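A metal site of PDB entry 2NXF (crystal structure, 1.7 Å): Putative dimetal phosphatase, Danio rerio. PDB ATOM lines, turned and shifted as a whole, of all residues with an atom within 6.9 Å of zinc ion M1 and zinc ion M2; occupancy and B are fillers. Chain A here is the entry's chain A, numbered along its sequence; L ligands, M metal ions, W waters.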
ATOM      1  N   ALA A  12       1.156  19.681   4.317  1.00  0.00           N
ATOM      2  CA  ALA A  12       2.110  20.322   3.394  1.00  0.00           C
ATOM      3  C   ALA A  12       1.968  21.832   3.405  1.00  0.00           C
ATOM      4  O   ALA A  12       0.856  22.356   3.513  1.00  0.00           O
ATOM      5  CB  ALA A  12       1.880  19.814   1.971  1.00  0.00           C
ATOM      6  N   ASP A  13       3.110  22.511   3.289  1.00  0.00           N
ATOM      7  CA  ASP A  13       3.148  23.941   2.888  1.00  0.00           C
ATOM      8  C   ASP A  13       2.357  24.815   3.862  1.00  0.00           C
ATOM      9  O   ASP A  13       1.499  25.617   3.458  1.00  0.00           O
ATOM     10  CB  ASP A  13       2.671  24.137   1.433  1.00  0.00           C
ATOM     11  CG  ASP A  13       3.632  23.480   0.426  1.00  0.00           C
ATOM     12  OD1 ASP A  13       4.501  24.174  -0.081  1.00  0.00           O
ATOM     13  OD2 ASP A  13       3.556  22.261   0.215  1.00  0.00           O
ATOM     14  N   VAL A  14       2.647  24.644   5.161  1.00  0.00           N
ATOM     15  CA  VAL A  14       2.069  25.514   6.207  1.00  0.00           C
ATOM     16  C   VAL A  14       2.454  26.979   5.890  1.00  0.00           C
ATOM     17  O   VAL A  14       1.601  27.865   5.832  1.00  0.00           O
ATOM     18  CB  VAL A  14       2.546  25.082   7.612  1.00  0.00           C
ATOM     19  CG1 VAL A  14       2.031  26.061   8.689  1.00  0.00           C
ATOM     20  CG2 VAL A  14       2.084  23.646   7.939  1.00  0.00           C
ATOM     21  N   GLN A  15       3.747  27.210   5.667  1.00  0.00           N
ATOM     22  CA  GLN A  15       4.258  28.510   5.223  1.00  0.00           C
ATOM     23  C   GLN A  15       3.827  29.658   6.128  1.00  0.00           C
ATOM     24  O   GLN A  15       3.452  30.738   5.659  1.00  0.00           O
ATOM     25  CB  GLN A  15       3.917  28.797   3.737  1.00  0.00           C
ATOM     26  CG  GLN A  15       5.111  28.477   2.864  1.00  0.00           C
ATOM     27  CD  GLN A  15       4.803  28.349   1.398  1.00  0.00           C
ATOM     28  OE1 GLN A  15       4.569  27.242   0.896  1.00  0.00           O
ATOM     29  NE2 GLN A  15       4.793  29.473   0.697  1.00  0.00           N
ATOM     30  N   ARG A  31      -2.802  33.873  -0.007  1.00  0.00           N
ATOM     31  CA  ARG A  31      -1.933  33.206   0.970  1.00  0.00           C
ATOM     32  C   ARG A  31      -2.255  33.672   2.401  1.00  0.00           C
ATOM     33  O   ARG A  31      -2.159  34.855   2.713  1.00  0.00           O
ATOM     34  CB  ARG A  31      -0.456  33.378   0.597  1.00  0.00           C
ATOM     35  CG  ARG A  31      -0.149  32.481  -0.590  1.00  0.00           C
ATOM     36  CD  ARG A  31       1.273  32.425  -1.023  1.00  0.00           C
ATOM     37  NE  ARG A  31       1.357  31.572  -2.215  1.00  0.00           N
ATOM     38  CZ  ARG A  31       2.483  31.055  -2.701  1.00  0.00           C
ATOM     39  NH1 ARG A  31       3.656  31.278  -2.092  1.00  0.00           N
ATOM     40  NH2 ARG A  31       2.429  30.310  -3.799  1.00  0.00           N
ATOM     41  N   LEU A  58       5.561  18.053   4.700  1.00  0.00           N
ATOM     42  CA  LEU A  58       6.174  17.993   3.384  1.00  0.00           C
ATOM     43  C   LEU A  58       6.968  19.255   2.989  1.00  0.00           C
ATOM     44  O   LEU A  58       7.382  19.391   1.833  1.00  0.00           O
ATOM     45  CB  LEU A  58       5.092  17.684   2.334  1.00  0.00           C
ATOM     46  CG  LEU A  58       4.723  16.193   2.102  1.00  0.00           C
ATOM     47  CD1 LEU A  58       5.934  15.428   1.529  1.00  0.00           C
ATOM     48  CD2 LEU A  58       4.271  15.548   3.361  1.00  0.00           C
ATOM     49  N   GLY A  59       7.221  20.154   3.956  1.00  0.00           N
ATOM     50  CA  GLY A  59       8.142  21.271   3.706  1.00  0.00           C
ATOM     51  C   GLY A  59       7.399  22.581   3.523  1.00  0.00           C
ATOM     52  O   GLY A  59       6.164  22.624   3.526  1.00  0.00           O
ATOM     53  N   ASP A  60       8.192  23.638   3.290  1.00  0.00           N
ATOM     54  CA  ASP A  60       7.701  25.009   3.302  1.00  0.00           C
ATOM     55  C   ASP A  60       6.914  25.253   4.573  1.00  0.00           C
ATOM     56  O   ASP A  60       5.803  25.793   4.518  1.00  0.00           O
ATOM     57  CB  ASP A  60       6.821  25.297   2.083  1.00  0.00           C
ATOM     58  CG  ASP A  60       7.607  25.429   0.782  1.00  0.00           C
ATOM     59  OD1 ASP A  60       8.851  25.317   0.790  1.00  0.00           O
ATOM     60  OD2 ASP A  60       6.981  25.579  -0.266  1.00  0.00           O
ATOM     61  N   ASP A  63       7.250  30.663   5.792  1.00  0.00           N
ATOM     62  CA  ASP A  63       7.409  31.350   4.504  1.00  0.00           C
ATOM     63  C   ASP A  63       8.751  32.067   4.403  1.00  0.00           C
ATOM     64  O   ASP A  63       9.272  32.554   5.415  1.00  0.00           O
ATOM     65  CB  ASP A  63       6.283  32.358   4.288  1.00  0.00           C
ATOM     66  CG  ASP A  63       6.143  32.772   2.843  1.00  0.00           C
ATOM     67  OD1 ASP A  63       5.544  31.995   2.067  1.00  0.00           O
ATOM     68  OD2 ASP A  63       6.653  33.830   2.482  1.00  0.00           O
ATOM     69  N   GLY A  95      11.843  22.040   1.939  1.00  0.00           N
ATOM     70  CA  GLY A  95      11.428  22.630   0.655  1.00  0.00           C
ATOM     71  C   GLY A  95      12.070  23.975   0.379  1.00  0.00           C
ATOM     72  O   GLY A  95      12.956  24.455   1.120  1.00  0.00           O
ATOM     73  N   ASN A  96      11.651  24.608  -0.712  1.00  0.00           N
ATOM     74  CA  ASN A  96      12.267  25.886  -1.108  1.00  0.00           C
ATOM     75  C   ASN A  96      12.232  26.966  -0.033  1.00  0.00           C
ATOM     76  O   ASN A  96      13.219  27.673   0.146  1.00  0.00           O
ATOM     77  CB  ASN A  96      11.807  26.419  -2.482  1.00  0.00           C
ATOM     78  CG  ASN A  96      10.295  26.481  -2.624  1.00  0.00           C
ATOM     79  OD1 ASN A  96       9.584  25.535  -2.303  1.00  0.00           O
ATOM     80  ND2 ASN A  96       9.803  27.624  -3.115  1.00  0.00           N
ATOM     81  N   HIS A  97      11.133  27.072   0.720  1.00  0.00           N
ATOM     82  CA  HIS A  97      11.036  28.119   1.746  1.00  0.00           C
ATOM     83  C   HIS A  97      11.954  27.899   2.932  1.00  0.00           C
ATOM     84  O   HIS A  97      12.411  28.859   3.566  1.00  0.00           O
ATOM     85  CB  HIS A  97       9.579  28.363   2.131  1.00  0.00           C
ATOM     86  CG  HIS A  97       8.830  29.110   1.077  1.00  0.00           C
ATOM     87  ND1 HIS A  97       8.626  30.471   1.144  1.00  0.00           N
ATOM     88  CD2 HIS A  97       8.324  28.713  -0.112  1.00  0.00           C
ATOM     89  CE1 HIS A  97       7.987  30.876   0.064  1.00  0.00           C
ATOM     90  NE2 HIS A  97       7.797  29.832  -0.718  1.00  0.00           N
ATOM     91  N   TYR A 100      15.096  29.464   1.644  1.00  0.00           N
ATOM     92  CA  TYR A 100      15.003  30.925   1.615  1.00  0.00           C
ATOM     93  C   TYR A 100      15.336  31.488   2.995  1.00  0.00           C
ATOM     94  O   TYR A 100      15.942  32.546   3.097  1.00  0.00           O
ATOM     95  CB  TYR A 100      13.598  31.412   1.236  1.00  0.00           C
ATOM     96  CG  TYR A 100      13.116  31.000  -0.148  1.00  0.00           C
ATOM     97  CD1 TYR A 100      14.013  30.773  -1.198  1.00  0.00           C
ATOM     98  CD2 TYR A 100      11.748  30.885  -0.405  1.00  0.00           C
ATOM     99  CE1 TYR A 100      13.559  30.393  -2.467  1.00  0.00           C
ATOM    100  CE2 TYR A 100      11.272  30.514  -1.666  1.00  0.00           C
ATOM    101  CZ  TYR A 100      12.182  30.258  -2.688  1.00  0.00           C
ATOM    102  OH  TYR A 100      11.704  29.858  -3.914  1.00  0.00           O
ATOM    103  N   TYR A 150      16.163  19.522  -3.259  1.00  0.00           N
ATOM    104  CA  TYR A 150      17.056  20.680  -3.518  1.00  0.00           C
ATOM    105  C   TYR A 150      18.541  20.322  -3.401  1.00  0.00           C
ATOM    106  O   TYR A 150      19.393  21.190  -3.262  1.00  0.00           O
ATOM    107  CB  TYR A 150      16.675  21.891  -2.634  1.00  0.00           C
ATOM    108  CG  TYR A 150      15.304  22.366  -3.009  1.00  0.00           C
ATOM    109  CD1 TYR A 150      15.125  23.367  -3.980  1.00  0.00           C
ATOM    110  CD2 TYR A 150      14.158  21.738  -2.482  1.00  0.00           C
ATOM    111  CE1 TYR A 150      13.853  23.767  -4.368  1.00  0.00           C
ATOM    112  CE2 TYR A 150      12.884  22.137  -2.861  1.00  0.00           C
ATOM    113  CZ  TYR A 150      12.731  23.132  -3.818  1.00  0.00           C
ATOM    114  OH  TYR A 150      11.487  23.554  -4.228  1.00  0.00           O
ATOM    115  N   PHE A 197      13.000  28.191  -8.084  1.00  0.00           N
ATOM    116  CA  PHE A 197      12.303  27.664  -6.905  1.00  0.00           C
ATOM    117  C   PHE A 197      12.122  26.135  -6.910  1.00  0.00           C
ATOM    118  O   PHE A 197      11.532  25.581  -5.994  1.00  0.00           O
ATOM    119  CB  PHE A 197      10.989  28.408  -6.645  1.00  0.00           C
ATOM    120  CG  PHE A 197       9.979  28.343  -7.763  1.00  0.00           C
ATOM    121  CD1 PHE A 197       9.123  27.233  -7.892  1.00  0.00           C
ATOM    122  CD2 PHE A 197       9.802  29.431  -8.626  1.00  0.00           C
ATOM    123  CE1 PHE A 197       8.122  27.186  -8.881  1.00  0.00           C
ATOM    124  CE2 PHE A 197       8.794  29.403  -9.634  1.00  0.00           C
ATOM    125  CZ  PHE A 197       7.965  28.289  -9.758  1.00  0.00           C
ATOM    126  N   ASN A 198      12.640  25.482  -7.952  1.00  0.00           N
ATOM    127  CA  ASN A 198      12.712  24.032  -8.008  1.00  0.00           C
ATOM    128  C   ASN A 198      14.154  23.528  -7.862  1.00  0.00           C
ATOM    129  O   ASN A 198      15.088  24.305  -7.640  1.00  0.00           O
ATOM    130  CB  ASN A 198      12.066  23.481  -9.282  1.00  0.00           C
ATOM    131  CG  ASN A 198      10.584  23.740  -9.333  1.00  0.00           C
ATOM    132  OD1 ASN A 198       9.931  23.901  -8.287  1.00  0.00           O
ATOM    133  ND2 ASN A 198      10.027  23.744 -10.536  1.00  0.00           N
ATOM    134  N   HIS A 228       9.730  17.243  -1.241  1.00  0.00           N
ATOM    135  CA  HIS A 228       8.951  18.487  -1.318  1.00  0.00           C
ATOM    136  C   HIS A 228       8.333  18.575  -2.726  1.00  0.00           C
ATOM    137  O   HIS A 228       7.175  18.993  -2.872  1.00  0.00           O
ATOM    138  CB  HIS A 228       9.803  19.729  -1.085  1.00  0.00           C
ATOM    139  CG  HIS A 228       8.998  20.976  -1.052  1.00  0.00           C
ATOM    140  ND1 HIS A 228       7.989  21.184  -0.130  1.00  0.00           N
ATOM    141  CD2 HIS A 228       9.016  22.072  -1.855  1.00  0.00           C
ATOM    142  CE1 HIS A 228       7.444  22.369  -0.357  1.00  0.00           C
ATOM    143  NE2 HIS A 228       8.048  22.923  -1.395  1.00  0.00           N
ATOM    144  N   LEU A 229       9.108  18.179  -3.725  1.00  0.00           N
ATOM    145  CA  LEU A 229       8.699  18.312  -5.126  1.00  0.00           C
ATOM    146  C   LEU A 229       8.082  17.041  -5.700  1.00  0.00           C
ATOM    147  O   LEU A 229       8.620  15.939  -5.523  1.00  0.00           O
ATOM    148  CB  LEU A 229       9.902  18.676  -6.016  1.00  0.00           C
ATOM    149  CG  LEU A 229      10.585  20.028  -5.715  1.00  0.00           C
ATOM    150  CD1 LEU A 229      11.783  20.240  -6.674  1.00  0.00           C
ATOM    151  CD2 LEU A 229       9.608  21.159  -5.798  1.00  0.00           C
ATOM    152  N   GLY A 264       4.622  17.901  -1.709  1.00  0.00           N
ATOM    153  CA  GLY A 264       3.873  19.149  -1.490  1.00  0.00           C
ATOM    154  C   GLY A 264       4.178  20.044  -2.673  1.00  0.00           C
ATOM    155  O   GLY A 264       4.167  19.596  -3.836  1.00  0.00           O
ATOM    156  N   HIS A 265       4.465  21.309  -2.382  1.00  0.00           N
ATOM    157  CA  HIS A 265       4.948  22.322  -3.355  1.00  0.00           C
ATOM    158  C   HIS A 265       3.860  22.872  -4.261  1.00  0.00           C
ATOM    159  O   HIS A 265       3.713  24.092  -4.362  1.00  0.00           O
ATOM    160  CB  HIS A 265       6.168  21.820  -4.161  1.00  0.00           C
ATOM    161  CG  HIS A 265       6.912  22.888  -4.909  1.00  0.00           C
ATOM    162  ND1 HIS A 265       7.541  23.954  -4.295  1.00  0.00           N
ATOM    163  CD2 HIS A 265       7.224  22.988  -6.225  1.00  0.00           C
ATOM    164  CE1 HIS A 265       8.177  24.680  -5.194  1.00  0.00           C
ATOM    165  NE2 HIS A 265       8.002  24.120  -6.387  1.00  0.00           N
ATOM    166  N   ASP A 266       3.129  21.994  -4.956  1.00  0.00           N
ATOM    167  CA  ASP A 266       2.009  22.480  -5.775  1.00  0.00           C
ATOM    168  C   ASP A 266       0.811  22.608  -4.842  1.00  0.00           C
ATOM    169  O   ASP A 266       0.169  21.600  -4.509  1.00  0.00           O
ATOM    170  CB  ASP A 266       1.715  21.490  -6.920  1.00  0.00           C
ATOM    171  CG  ASP A 266       0.578  21.928  -7.813  1.00  0.00           C
ATOM    172  OD1 ASP A 266      -0.109  22.931  -7.499  1.00  0.00           O
ATOM    173  OD2 ASP A 266       0.379  21.284  -8.860  1.00  0.00           O
ATOM    174  N   HIS A 267       0.513  23.840  -4.423  1.00  0.00           N
ATOM    175  CA  HIS A 267      -0.508  24.062  -3.378  1.00  0.00           C
ATOM    176  C   HIS A 267      -1.906  23.652  -3.814  1.00  0.00           C
ATOM    177  O   HIS A 267      -2.779  23.476  -2.983  1.00  0.00           O
ATOM    178  CB  HIS A 267      -0.535  25.526  -2.939  1.00  0.00           C
ATOM    179  CG  HIS A 267       0.781  26.022  -2.410  1.00  0.00           C
ATOM    180  ND1 HIS A 267       1.140  27.361  -2.433  1.00  0.00           N
ATOM    181  CD2 HIS A 267       1.812  25.360  -1.824  1.00  0.00           C
ATOM    182  CE1 HIS A 267       2.340  27.493  -1.896  1.00  0.00           C
ATOM    183  NE2 HIS A 267       2.777  26.298  -1.517  1.00  0.00           N
ATOM    184  N   GLY A 285      -1.972  22.602  -0.338  1.00  0.00           N
ATOM    185  CA  GLY A 285      -1.128  23.360   0.607  1.00  0.00           C
ATOM    186  C   GLY A 285      -1.950  24.147   1.602  1.00  0.00           C
ATOM    187  O   GLY A 285      -2.939  24.823   1.253  1.00  0.00           O
ATOM    188  N   ILE A 287      -1.078  26.820   3.166  1.00  0.00           N
ATOM    189  CA  ILE A 287      -0.977  28.280   2.978  1.00  0.00           C
ATOM    190  C   ILE A 287      -2.053  28.877   2.083  1.00  0.00           C
ATOM    191  O   ILE A 287      -2.462  30.017   2.299  1.00  0.00           O
ATOM    192  CB  ILE A 287       0.441  28.686   2.520  1.00  0.00           C
ATOM    193  CG1 ILE A 287       0.618  30.213   2.503  1.00  0.00           C
ATOM    194  CG2 ILE A 287       0.781  28.068   1.149  1.00  0.00           C
ATOM    195  CD1 ILE A 287       0.480  30.871   3.879  1.00  0.00           C
HETATM  196  P1  LIG L   1       5.972  28.148  -3.107  1.00  0.00           P
HETATM  197  O1  LIG L   1       5.018  27.864  -4.252  1.00  0.00           O
HETATM  198  O2  LIG L   1       6.381  29.601  -3.153  1.00  0.00           O
HETATM  199  O3  LIG L   1       5.289  27.991  -1.750  1.00  0.00           O
HETATM  200  O4  LIG L   1       7.148  27.233  -3.145  1.00  0.00           O
HETATM  201 ZN    ZN M   1       7.545  24.893  -2.255  1.00  0.00          ZN
HETATM  202 ZN    ZN M   2       4.869  26.109  -0.715  1.00  0.00          ZN
HETATM  203  O   HOH W   1       5.474  25.315  -2.621  1.00  0.00           O
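The side-chain amide oxygen (OD1) of Asn 96 is bound to zinc ion M1, 2.1 Å away.
Zinc ion M1 is bound by water W1 (2.1 Å).
Zinc ion M1 is bound by OD2 of Asp 60, at 2.2 Å.
A ring nitrogen (NE2) of His 228 binds zinc ion M1.
ND1 of His 265 binds zinc ion M1 (2.2 Å).
Zinc ion M1 is bound by O4 of the ligand.
OE1 of Gln 15 binds zinc ion M2 (2.0 Å).
OD1 of Asp 13 is bound to zinc ion M2, 2.1 Å away.
Zinc ion M2 is bound by water W1, at 2.2 Å.
O3 of the ligand binds zinc ion M2 (2.2 Å).
OD2 of Asp 60 binds zinc ion M2 (2.2 Å).
NE2 of His 267 binds zinc ion M2, 2.2 Å away.
Zinc ion M2 has six donor atoms within binding distance.
The side-chain carboxylate (OD2) of Asp 13 is in hydrogen-bond range of the backbone NH (N) of His 265.
N of Ile 287 is in hydrogen-bond range of O of Asp 13.
N of Asp 13 sits at hydrogen-bond distance from O of Gly 59.
The side-chain hydroxyl of Tyr 100 lies within hydrogen-bond range of the side-chain amide nitrogen of Asn 96 (3.0 Å).
The side-chain carboxylate (OD1) of Asp 60 sits at hydrogen-bond distance from the backbone NH (N) of His 97 (2.9 Å).
The backbone carbonyl oxygen of Asp 60 sits at hydrogen-bond distance from the backbone NH of Val 14, 3.4 Å away.
ND1 of His 228 sits at hydrogen-bond distance from O of Leu 58 (2.7 Å).
The guanidinium group (NH2) of Arg 31 sits close to a ring nitrogen (ND1) of His 267.
Four residues have an atom within 4 Å of zinc ion M2: Asp 13, Gln 15, Asp 60 and His 267.
Along chain A the residues within 4 Å of zinc ion M1 span positions 13 to 265.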
